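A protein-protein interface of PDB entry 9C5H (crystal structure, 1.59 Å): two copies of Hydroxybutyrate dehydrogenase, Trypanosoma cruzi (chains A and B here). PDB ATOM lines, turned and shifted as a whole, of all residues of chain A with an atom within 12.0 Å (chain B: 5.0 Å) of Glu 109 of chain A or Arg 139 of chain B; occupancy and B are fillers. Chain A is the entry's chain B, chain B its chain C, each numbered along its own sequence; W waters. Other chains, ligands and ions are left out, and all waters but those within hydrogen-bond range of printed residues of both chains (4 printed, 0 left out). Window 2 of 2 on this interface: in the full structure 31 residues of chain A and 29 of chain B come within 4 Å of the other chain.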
ATOM      1  N   HIS A 104       5.115   6.620  -6.421  1.00  0.00           N
ATOM      2  CA  HIS A 104       5.079   8.066  -6.618  1.00  0.00           C
ATOM      3  C   HIS A 104       3.936   8.629  -5.791  1.00  0.00           C
ATOM      4  O   HIS A 104       2.781   8.243  -5.992  1.00  0.00           O
ATOM      5  CB  HIS A 104       4.894   8.464  -8.077  1.00  0.00           C
ATOM      6  CG  HIS A 104       4.927   9.948  -8.288  1.00  0.00           C
ATOM      7  ND1 HIS A 104       6.104  10.653  -8.410  1.00  0.00           N
ATOM      8  CD2 HIS A 104       3.932  10.865  -8.357  1.00  0.00           C
ATOM      9  CE1 HIS A 104       5.833  11.937  -8.570  1.00  0.00           C
ATOM     10  NE2 HIS A 104       4.522  12.093  -8.538  1.00  0.00           N
ATOM     11  N   VAL A 105       4.259   9.559  -4.895  1.00  0.00           N
ATOM     12  CA  VAL A 105       3.305  10.127  -3.949  1.00  0.00           C
ATOM     13  C   VAL A 105       2.791  11.448  -4.514  1.00  0.00           C
ATOM     14  O   VAL A 105       3.578  12.356  -4.811  1.00  0.00           O
ATOM     15  CB  VAL A 105       3.954  10.326  -2.569  1.00  0.00           C
ATOM     16  CG1 VAL A 105       2.981  10.989  -1.610  1.00  0.00           C
ATOM     17  CG2 VAL A 105       4.454   8.987  -2.004  1.00  0.00           C
ATOM     18  N   SER A 106       1.470  11.552  -4.668  1.00  0.00           N
ATOM     19  CA  SER A 106       0.826  12.744  -5.209  1.00  0.00           C
ATOM     20  C   SER A 106      -0.673  12.665  -4.965  1.00  0.00           C
ATOM     21  O   SER A 106      -1.255  11.582  -5.100  1.00  0.00           O
ATOM     22  CB  SER A 106       1.069  12.881  -6.713  1.00  0.00           C
ATOM     23  OG  SER A 106       0.291  13.938  -7.260  1.00  0.00           O
ATOM     24  N   PRO A 107      -1.340  13.778  -4.654  1.00  0.00           N
ATOM     25  CA  PRO A 107      -2.808  13.774  -4.675  1.00  0.00           C
ATOM     26  C   PRO A 107      -3.300  13.398  -6.063  1.00  0.00           C
ATOM     27  O   PRO A 107      -2.592  13.557  -7.060  1.00  0.00           O
ATOM     28  CB  PRO A 107      -3.191  15.219  -4.326  1.00  0.00           C
ATOM     29  CG  PRO A 107      -1.951  15.851  -3.811  1.00  0.00           C
ATOM     30  CD  PRO A 107      -0.787  15.120  -4.402  1.00  0.00           C
ATOM     31  N   VAL A 108      -4.538  12.904  -6.127  1.00  0.00           N
ATOM     32  CA  VAL A 108      -5.061  12.422  -7.402  1.00  0.00           C
ATOM     33  C   VAL A 108      -5.132  13.541  -8.429  1.00  0.00           C
ATOM     34  O   VAL A 108      -4.923  13.313  -9.625  1.00  0.00           O
ATOM     35  CB  VAL A 108      -6.443  11.775  -7.221  1.00  0.00           C
ATOM     36  CG1 VAL A 108      -7.075  11.495  -8.579  1.00  0.00           C
ATOM     37  CG2 VAL A 108      -6.315  10.510  -6.457  1.00  0.00           C
ATOM     38  N   GLU A 109      -5.489  14.756  -7.996  1.00  0.00           N
ATOM     39  CA  GLU A 109      -5.764  15.809  -8.968  1.00  0.00           C
ATOM     40  C   GLU A 109      -4.541  16.147  -9.803  1.00  0.00           C
ATOM     41  O   GLU A 109      -4.670  16.567 -10.959  1.00  0.00           O
ATOM     42  CB  GLU A 109      -6.235  17.084  -8.273  1.00  0.00           C
ATOM     43  CG  GLU A 109      -7.588  16.998  -7.625  1.00  0.00           C
ATOM     44  CD  GLU A 109      -7.564  16.383  -6.235  1.00  0.00           C
ATOM     45  OE1 GLU A 109      -6.492  15.966  -5.746  1.00  0.00           O
ATOM     46  OE2 GLU A 109      -8.648  16.319  -5.626  1.00  0.00           O
ATOM     47  N   THR A 110      -3.355  16.034  -9.217  1.00  0.00           N
ATOM     48  CA  THR A 110      -2.120  16.420  -9.879  1.00  0.00           C
ATOM     49  C   THR A 110      -1.236  15.224 -10.184  1.00  0.00           C
ATOM     50  O   THR A 110      -0.066  15.403 -10.535  1.00  0.00           O
ATOM     51  CB  THR A 110      -1.365  17.433  -9.019  1.00  0.00           C
ATOM     52  OG1 THR A 110      -1.189  16.903  -7.700  1.00  0.00           O
ATOM     53  CG2 THR A 110      -2.148  18.733  -8.950  1.00  0.00           C
ATOM     54  N   PHE A 111      -1.767  14.018 -10.072  1.00  0.00           N
ATOM     55  CA  PHE A 111      -0.970  12.831 -10.322  1.00  0.00           C
ATOM     56  C   PHE A 111      -0.537  12.829 -11.783  1.00  0.00           C
ATOM     57  O   PHE A 111      -1.398  12.813 -12.674  1.00  0.00           O
ATOM     58  CB  PHE A 111      -1.761  11.570  -9.998  1.00  0.00           C
ATOM     59  CG  PHE A 111      -0.899  10.443  -9.537  1.00  0.00           C
ATOM     60  CD1 PHE A 111      -0.109   9.751 -10.438  1.00  0.00           C
ATOM     61  CD2 PHE A 111      -0.845  10.097  -8.199  1.00  0.00           C
ATOM     62  CE1 PHE A 111       0.710   8.725 -10.013  1.00  0.00           C
ATOM     63  CE2 PHE A 111      -0.029   9.071  -7.767  1.00  0.00           C
ATOM     64  CZ  PHE A 111       0.749   8.384  -8.674  1.00  0.00           C
ATOM     65  N   PRO A 112       0.778  12.848 -12.080  1.00  0.00           N
ATOM     66  CA  PRO A 112       1.212  12.912 -13.460  1.00  0.00           C
ATOM     67  C   PRO A 112       0.719  11.715 -14.239  1.00  0.00           C
ATOM     68  O   PRO A 112       0.839  10.607 -13.741  1.00  0.00           O
ATOM     69  CB  PRO A 112       2.737  12.966 -13.334  1.00  0.00           C
ATOM     70  CG  PRO A 112       2.981  13.493 -11.949  1.00  0.00           C
ATOM     71  CD  PRO A 112       1.883  12.851 -11.136  1.00  0.00           C
ATOM     72  N   SER A 113       0.210  11.937 -15.447  1.00  0.00           N
ATOM     73  CA  SER A 113      -0.363  10.831 -16.270  1.00  0.00           C
ATOM     74  C   SER A 113       0.700   9.745 -16.566  1.00  0.00           C
ATOM     75  O   SER A 113       0.440   8.509 -16.688  1.00  0.00           O
ATOM     76  CB  SER A 113      -1.040  11.372 -17.543  1.00  0.00           C
ATOM     77  OG  SER A 113      -1.544  10.315 -18.346  1.00  0.00           O
ATOM     78  N   ASP A 114       1.911  10.202 -16.869  1.00  0.00           N
ATOM     79  CA  ASP A 114       2.997   9.226 -17.181  1.00  0.00           C
ATOM     80  C   ASP A 114       3.457   8.410 -15.956  1.00  0.00           C
ATOM     81  O   ASP A 114       4.029   7.289 -16.033  1.00  0.00           O
ATOM     82  CB  ASP A 114       4.192   9.903 -17.835  1.00  0.00           C
ATOM     83  CG  ASP A 114       4.868  10.974 -16.997  1.00  0.00           C
ATOM     84  OD1 ASP A 114       4.327  11.279 -15.920  1.00  0.00           O
ATOM     85  OD2 ASP A 114       5.923  11.480 -17.429  1.00  0.00           O
ATOM     86  N   LYS A 115       3.367   9.026 -14.784  1.00  0.00           N
ATOM     87  CA  LYS A 115       3.743   8.320 -13.535  1.00  0.00           C
ATOM     88  C   LYS A 115       2.654   7.287 -13.220  1.00  0.00           C
ATOM     89  O   LYS A 115       3.003   6.235 -12.702  1.00  0.00           O
ATOM     90  CB  LYS A 115       3.903   9.274 -12.354  1.00  0.00           C
ATOM     91  CG  LYS A 115       5.108  10.187 -12.414  1.00  0.00           C
ATOM     92  CD  LYS A 115       6.436   9.449 -12.335  1.00  0.00           C
ATOM     93  CE  LYS A 115       7.583  10.400 -12.343  1.00  0.00           C
ATOM     94  NZ  LYS A 115       8.649   9.929 -13.229  1.00  0.00           N
ATOM     95  N   TRP A 116       1.392   7.593 -13.517  1.00  0.00           N
ATOM     96  CA  TRP A 116       0.327   6.636 -13.315  1.00  0.00           C
ATOM     97  C   TRP A 116       0.568   5.462 -14.240  1.00  0.00           C
ATOM     98  O   TRP A 116       0.587   4.346 -13.825  1.00  0.00           O
ATOM     99  CB  TRP A 116      -1.060   7.246 -13.607  1.00  0.00           C
ATOM    100  CG  TRP A 116      -2.155   6.227 -13.668  1.00  0.00           C
ATOM    101  CD1 TRP A 116      -2.387   5.378 -14.660  1.00  0.00           C
ATOM    102  CD2 TRP A 116      -3.139   5.932 -12.665  1.00  0.00           C
ATOM    103  NE1 TRP A 116      -3.428   4.571 -14.373  1.00  0.00           N
ATOM    104  CE2 TRP A 116      -3.916   4.901 -13.150  1.00  0.00           C
ATOM    105  CE3 TRP A 116      -3.468   6.480 -11.446  1.00  0.00           C
ATOM    106  CZ2 TRP A 116      -4.948   4.362 -12.428  1.00  0.00           C
ATOM    107  CZ3 TRP A 116      -4.488   5.942 -10.741  1.00  0.00           C
ATOM    108  CH2 TRP A 116      -5.204   4.893 -11.219  1.00  0.00           C
ATOM    109  N   SER A 158      -4.436   4.287   0.836  1.00  0.00           N
ATOM    110  CA  SER A 158      -3.754   5.352   1.563  1.00  0.00           C
ATOM    111  C   SER A 158      -3.758   6.621   0.720  1.00  0.00           C
ATOM    112  O   SER A 158      -3.624   6.562  -0.505  1.00  0.00           O
ATOM    113  CB  SER A 158      -2.303   4.982   1.904  1.00  0.00           C
ATOM    114  OG  SER A 158      -2.247   3.846   2.744  1.00  0.00           O
ATOM    115  N   MET A 159      -3.872   7.767   1.383  1.00  0.00           N
ATOM    116  CA  MET A 159      -3.886   9.037   0.668  1.00  0.00           C
ATOM    117  C   MET A 159      -2.624   9.217  -0.166  1.00  0.00           C
ATOM    118  O   MET A 159      -1.524   8.835   0.245  1.00  0.00           O
ATOM    119  CB  MET A 159      -4.014  10.193   1.656  1.00  0.00           C
ATOM    120  CG  MET A 159      -5.378  10.290   2.289  1.00  0.00           C
ATOM    121  SD  MET A 159      -5.596  11.784   3.264  1.00  0.00           S
ATOM    122  CE  MET A 159      -4.709  11.370   4.763  1.00  0.00           C
ATOM    123  N   ASN A 160      -2.800   9.800  -1.354  1.00  0.00           N
ATOM    124  CA  ASN A 160      -1.715  10.231  -2.229  1.00  0.00           C
ATOM    125  C   ASN A 160      -0.967   9.075  -2.868  1.00  0.00           C
ATOM    126  O   ASN A 160       0.139   9.262  -3.382  1.00  0.00           O
ATOM    127  CB  ASN A 160      -0.758  11.141  -1.457  1.00  0.00           C
ATOM    128  CG  ASN A 160      -1.472  12.335  -0.863  1.00  0.00           C
ATOM    129  OD1 ASN A 160      -2.350  12.916  -1.502  1.00  0.00           O
ATOM    130  ND2 ASN A 160      -1.135  12.683   0.372  1.00  0.00           N
ATOM    131  N   LYS A 161      -1.585   7.897  -2.907  1.00  0.00           N
ATOM    132  CA  LYS A 161      -0.992   6.700  -3.497  1.00  0.00           C
ATOM    133  C   LYS A 161      -1.987   6.000  -4.411  1.00  0.00           C
ATOM    134  O   LYS A 161      -2.071   4.767  -4.447  1.00  0.00           O
ATOM    135  CB  LYS A 161      -0.482   5.770  -2.400  1.00  0.00           C
ATOM    136  CG  LYS A 161       0.739   6.351  -1.693  1.00  0.00           C
ATOM    137  CD  LYS A 161       1.207   5.515  -0.515  1.00  0.00           C
ATOM    138  CE  LYS A 161       2.478   6.103   0.094  1.00  0.00           C
ATOM    139  NZ  LYS A 161       2.987   5.302   1.242  1.00  0.00           N
ATOM    140  N   SER A 162      -2.716   6.783  -5.208  1.00  0.00           N
ATOM    141  CA  SER A 162      -3.798   6.223  -6.014  1.00  0.00           C
ATOM    142  C   SER A 162      -3.280   5.210  -7.030  1.00  0.00           C
ATOM    143  O   SER A 162      -3.824   4.107  -7.147  1.00  0.00           O
ATOM    144  CB  SER A 162      -4.572   7.344  -6.714  1.00  0.00           C
ATOM    145  OG  SER A 162      -3.743   8.130  -7.556  1.00  0.00           O
ATOM    146  N   ALA A 163      -2.241   5.562  -7.792  1.00  0.00           N
ATOM    147  CA  ALA A 163      -1.770   4.630  -8.814  1.00  0.00           C
ATOM    148  C   ALA A 163      -1.215   3.362  -8.182  1.00  0.00           C
ATOM    149  O   ALA A 163      -1.438   2.253  -8.681  1.00  0.00           O
ATOM    150  CB  ALA A 163      -0.698   5.274  -9.693  1.00  0.00           C
ATOM    151  N   GLN B 132      -9.781  12.565 -12.158  1.00  0.00           N
ATOM    152  CA  GLN B 132      -8.835  13.669 -12.083  1.00  0.00           C
ATOM    153  C   GLN B 132      -9.418  14.935 -12.684  1.00  0.00           C
ATOM    154  O   GLN B 132      -9.237  16.033 -12.144  1.00  0.00           O
ATOM    155  CB  GLN B 132      -7.564  13.263 -12.811  1.00  0.00           C
ATOM    156  CG  GLN B 132      -6.466  14.248 -12.737  1.00  0.00           C
ATOM    157  CD  GLN B 132      -5.187  13.659 -13.254  1.00  0.00           C
ATOM    158  OE1 GLN B 132      -5.061  13.377 -14.444  1.00  0.00           O
ATOM    159  NE2 GLN B 132      -4.239  13.435 -12.357  1.00  0.00           N
ATOM    160  N   LEU B 135     -12.593  16.269 -10.233  1.00  0.00           N
ATOM    161  CA  LEU B 135     -12.445  16.578  -8.814  1.00  0.00           C
ATOM    162  C   LEU B 135     -12.237  18.060  -8.513  1.00  0.00           C
ATOM    163  O   LEU B 135     -12.807  18.539  -7.518  1.00  0.00           O
ATOM    164  CB  LEU B 135     -11.292  15.753  -8.227  1.00  0.00           C
ATOM    165  CG  LEU B 135     -11.618  14.331  -7.763  1.00  0.00           C
ATOM    166  CD1 LEU B 135     -10.333  13.578  -7.454  1.00  0.00           C
ATOM    167  CD2 LEU B 135     -12.540  14.348  -6.549  1.00  0.00           C
ATOM    168  N   PRO B 136     -11.422  18.816  -9.258  1.00  0.00           N
ATOM    169  CA  PRO B 136     -11.220  20.229  -8.877  1.00  0.00           C
ATOM    170  C   PRO B 136     -12.512  21.020  -8.794  1.00  0.00           C
ATOM    171  O   PRO B 136     -12.709  21.797  -7.847  1.00  0.00           O
ATOM    172  CB  PRO B 136     -10.289  20.751  -9.980  1.00  0.00           C
ATOM    173  CG  PRO B 136      -9.475  19.525 -10.355  1.00  0.00           C
ATOM    174  CD  PRO B 136     -10.479  18.384 -10.309  1.00  0.00           C
ATOM    175  N   SER B 137     -13.416  20.819  -9.752  1.00  0.00           N
ATOM    176  CA  SER B 137     -14.706  21.493  -9.711  1.00  0.00           C
ATOM    177  C   SER B 137     -15.518  21.045  -8.507  1.00  0.00           C
ATOM    178  O   SER B 137     -16.134  21.864  -7.814  1.00  0.00           O
ATOM    179  CB  SER B 137     -15.478  21.213 -10.998  1.00  0.00           C
ATOM    180  OG  SER B 137     -16.773  21.786 -10.946  1.00  0.00           O
ATOM    181  N   MET B 138     -15.544  19.738  -8.252  1.00  0.00           N
ATOM    182  CA  MET B 138     -16.309  19.232  -7.120  1.00  0.00           C
ATOM    183  C   MET B 138     -15.803  19.829  -5.816  1.00  0.00           C
ATOM    184  O   MET B 138     -16.597  20.180  -4.938  1.00  0.00           O
ATOM    185  CB  MET B 138     -16.234  17.708  -7.080  1.00  0.00           C
ATOM    186  CG  MET B 138     -16.989  17.025  -8.194  1.00  0.00           C
ATOM    187  SD  MET B 138     -16.685  15.248  -8.191  1.00  0.00           S
ATOM    188  CE  MET B 138     -17.803  14.767  -9.499  1.00  0.00           C
ATOM    189  N   ARG B 139     -14.482  19.961  -5.672  1.00  0.00           N
ATOM    190  CA  ARG B 139     -13.945  20.559  -4.454  1.00  0.00           C
ATOM    191  C   ARG B 139     -14.368  22.017  -4.330  1.00  0.00           C
ATOM    192  O   ARG B 139     -14.727  22.478  -3.240  1.00  0.00           O
ATOM    193  CB  ARG B 139     -12.422  20.445  -4.435  1.00  0.00           C
ATOM    194  CG  ARG B 139     -11.886  19.040  -4.203  1.00  0.00           C
ATOM    195  CD  ARG B 139     -10.376  19.080  -4.064  1.00  0.00           C
ATOM    196  NE  ARG B 139      -9.813  17.781  -3.719  1.00  0.00           N
ATOM    197  CZ  ARG B 139      -9.761  17.294  -2.487  1.00  0.00           C
ATOM    198  NH1 ARG B 139     -10.314  17.933  -1.468  1.00  0.00           N
ATOM    199  NH2 ARG B 139      -9.139  16.136  -2.273  1.00  0.00           N
ATOM    200  N   GLN B 140     -14.330  22.757  -5.440  1.00  0.00           N
ATOM    201  CA  GLN B 140     -14.751  24.152  -5.412  1.00  0.00           C
ATOM    202  C   GLN B 140     -16.214  24.278  -5.022  1.00  0.00           C
ATOM    203  O   GLN B 140     -16.599  25.216  -4.313  1.00  0.00           O
ATOM    204  CB  GLN B 140     -14.551  24.793  -6.778  1.00  0.00           C
ATOM    205  CG  GLN B 140     -13.172  25.239  -7.078  1.00  0.00           C
ATOM    206  CD  GLN B 140     -13.147  26.088  -8.320  1.00  0.00           C
ATOM    207  OE1 GLN B 140     -13.387  25.595  -9.421  1.00  0.00           O
ATOM    208  NE2 GLN B 140     -12.896  27.380  -8.150  1.00  0.00           N
ATOM    209  N   ARG B 141     -17.052  23.371  -5.523  1.00  0.00           N
ATOM    210  CA  ARG B 141     -18.488  23.425  -5.296  1.00  0.00           C
ATOM    211  C   ARG B 141     -18.908  22.786  -3.982  1.00  0.00           C
ATOM    212  O   ARG B 141     -20.066  22.949  -3.582  1.00  0.00           O
ATOM    213  CB  ARG B 141     -19.211  22.747  -6.461  1.00  0.00           C
ATOM    214  CG  ARG B 141     -19.009  23.468  -7.783  1.00  0.00           C
ATOM    215  CD  ARG B 141     -19.789  22.819  -8.907  1.00  0.00           C
ATOM    216  NE  ARG B 141     -21.187  23.229  -8.976  1.00  0.00           N
ATOM    217  CZ  ARG B 141     -21.639  24.237  -9.712  1.00  0.00           C
ATOM    218  NH1 ARG B 141     -20.815  25.062 -10.336  1.00  0.00           N
ATOM    219  NH2 ARG B 141     -22.951  24.413  -9.836  1.00  0.00           N
ATOM    220  N   GLY B 142     -18.006  22.078  -3.307  1.00  0.00           N
ATOM    221  CA  GLY B 142     -18.308  21.506  -2.013  1.00  0.00           C
ATOM    222  C   GLY B 142     -19.136  20.247  -2.050  1.00  0.00           C
ATOM    223  O   GLY B 142     -19.691  19.851  -1.021  1.00  0.00           O
ATOM    224  N   GLU B 181      -8.749  10.788   0.198  1.00  0.00           N
ATOM    225  CA  GLU B 181      -8.258  12.132  -0.101  1.00  0.00           C
ATOM    226  C   GLU B 181      -9.359  13.181  -0.039  1.00  0.00           C
ATOM    227  O   GLU B 181      -9.048  14.378   0.065  1.00  0.00           O
ATOM    228  CB  GLU B 181      -7.600  12.171  -1.487  1.00  0.00           C
ATOM    229  CG  GLU B 181      -6.303  11.383  -1.569  1.00  0.00           C
ATOM    230  CD  GLU B 181      -5.601  11.471  -2.914  1.00  0.00           C
ATOM    231  OE1 GLU B 181      -5.908  12.379  -3.718  1.00  0.00           O
ATOM    232  OE2 GLU B 181      -4.719  10.619  -3.157  1.00  0.00           O
ATOM    233  N   THR B 182     -10.628  12.771  -0.106  1.00  0.00           N
ATOM    234  CA  THR B 182     -11.764  13.684  -0.039  1.00  0.00           C
ATOM    235  C   THR B 182     -12.608  13.499   1.220  1.00  0.00           C
ATOM    236  O   THR B 182     -13.719  14.039   1.292  1.00  0.00           O
ATOM    237  CB  THR B 182     -12.675  13.514  -1.265  1.00  0.00           C
ATOM    238  OG1 THR B 182     -13.133  12.154  -1.352  1.00  0.00           O
ATOM    239  CG2 THR B 182     -11.963  13.889  -2.548  1.00  0.00           C
ATOM    240  N   THR B 185     -14.594  16.320   2.986  1.00  0.00           N
ATOM    241  CA  THR B 185     -15.337  17.195   2.098  1.00  0.00           C
ATOM    242  C   THR B 185     -16.710  16.600   1.805  1.00  0.00           C
ATOM    243  O   THR B 185     -17.032  15.477   2.205  1.00  0.00           O
ATOM    244  CB  THR B 185     -14.617  17.404   0.761  1.00  0.00           C
ATOM    245  OG1 THR B 185     -14.774  16.220  -0.039  1.00  0.00           O
ATOM    246  CG2 THR B 185     -13.144  17.703   0.946  1.00  0.00           C
ATOM    247  N   ILE B 187     -17.470  15.497  -1.015  1.00  0.00           N
ATOM    248  CA  ILE B 187     -17.259  14.580  -2.130  1.00  0.00           C
ATOM    249  C   ILE B 187     -17.083  13.177  -1.570  1.00  0.00           C
ATOM    250  O   ILE B 187     -16.253  12.964  -0.678  1.00  0.00           O
ATOM    251  CB  ILE B 187     -16.019  14.972  -2.950  1.00  0.00           C
ATOM    252  CG1 ILE B 187     -16.103  16.414  -3.441  1.00  0.00           C
ATOM    253  CG2 ILE B 187     -15.820  13.983  -4.100  1.00  0.00           C
ATOM    254  CD1 ILE B 187     -14.748  16.937  -3.876  1.00  0.00           C
HETATM  255  O   HOH W   1      -8.607  13.805   3.466  1.00  0.00           O
HETATM  256  O   HOH W   2      -6.764  14.884  -3.464  1.00  0.00           O
HETATM  257  O   HOH W   3      -7.219  17.779 -12.413  1.00  0.00           O
HETATM  258  O   HOH W   4      -3.235   9.788  -5.276  1.00  0.00           O
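The side-chain amide nitrogen (NE2) of Gln 132 of chain B sits at hydrogen-bond distance from the backbone carbonyl oxygen (O) of Val 108 of chain A (2.8 Å). The backbone NH (N) of Val 108 of chain A is in hydrogen-bond range of the side-chain carboxylate (OE1) of Glu 181 of chain B (2.8 Å). O of Phe 111 of chain A is in hydrogen-bond range of NE2 of Gln 132 of chain B, at 2.9 Å. The backbone NH (N) of Asn 160 of chain A sits at hydrogen-bond distance from the side-chain carboxylate (OE2) of Glu 181 of chain B, at 2.8 Å. The side-chain carboxylate (OE2) of Glu 109 of chain A lies within salt-bridge range of the guanidinium group (NE) of Arg 139 of chain B, at 2.7 Å. NE2 of Gln 132 of chain B lies close to O of Glu 109 of chain A (3.5 Å).
The backbone NH of Ser 106 of chain A lies within hydrogen-bond range of the backbone carbonyl oxygen of Asn 160 of chain A (2.9 Å). The guanidinium group (NH2) of Arg 139 of chain B sits at hydrogen-bond distance from the backbone carbonyl oxygen (O) of Glu 181 of chain B. The side-chain hydroxyl (OG) of Ser 106 of chain A is in hydrogen-bond range of the backbone NH (N) of Phe 111 of chain A, at 3.5 Å.
Hydrophobic or aromatic side chains of chain A that line the printed part of chain B: Pro 107, Val 108, Phe 111 and Met 159.
No position is printed for both chains.
Water W2 lies within hydrogen-bond range of OE1 of Glu 109 of chain A, OE1 of Glu 181 of chain B and NH2 of Arg 139 of chain B. Water W4 lies within hydrogen-bond range of the backbone carbonyl oxygen of Ser 106 of chain A, the side-chain carboxylate of Glu 181 of chain B, the side-chain hydroxyl of Ser 162 of chain A, the backbone NH of Lys 161 of chain A and the backbone NH of Val 108 of chain A. Water W3 bridges O of Gln 132 of chain B (2.7 Å) and O of Glu 109 of chain A (3.2 Å). Water W1 bridges the backbone carbonyl oxygen of Glu 181 of chain B (3.5 Å) and the side-chain sulfur of Met 159 of chain A (3.6 Å).
Among the printed residues, pairs that only touch across the chains: Pro 107 of chain A with Glu 181 of chain B (3.5 Å), Glu 109 of chain A with Leu 135 of chain B (3.7 Å) and Met 159 of chain A with Glu 181 of chain B (3.9 Å).
Of the printed residues of chain B, Glu 109 of chain A touches Gln 132, Leu 135 and Arg 139. Of chain A, only Glu 109 comes within 4 Å of Arg 139 of chain B. Gln 132 of chain B touches just these residues of chain A: Val 108, Glu 109 and Phe 111. Of chain A, only Glu 109 comes within 4 Å of Leu 135 of chain B. No residue of chain A comes within 4 Å of Pro 136 of chain B. No residue of chain A comes within 4 Å of Met 138 of chain B. No residue of chain A comes within 4 Å of Gln 140 of chain B. No residue of chain A comes within 4 Å of Gly 142 of chain B. No residue of chain A comes within 4 Å of Thr 182 of chain B. Of the printed residues of chain B, Asn 160 of chain A touches Glu 181 (2.8 Å). Printed residues of chain B within 4 Å of Met 159 of chain A: Glu 181 (3.9 Å). Printed residues of chain B within 4 Å of Pro 107 of chain A: Glu 181. Printed residues of chain B within 4 Å of Phe 111 of chain A: Gln 132. Printed residues of chain B within 4 Å of Val 108 of chain A: Gln 132 (2.8 Å) and Glu 181 (2.8 Å). The nearest printed residue of chain B that does not touch Glu 109 of chain A is Glu 181 of chain B (4.2 Å).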
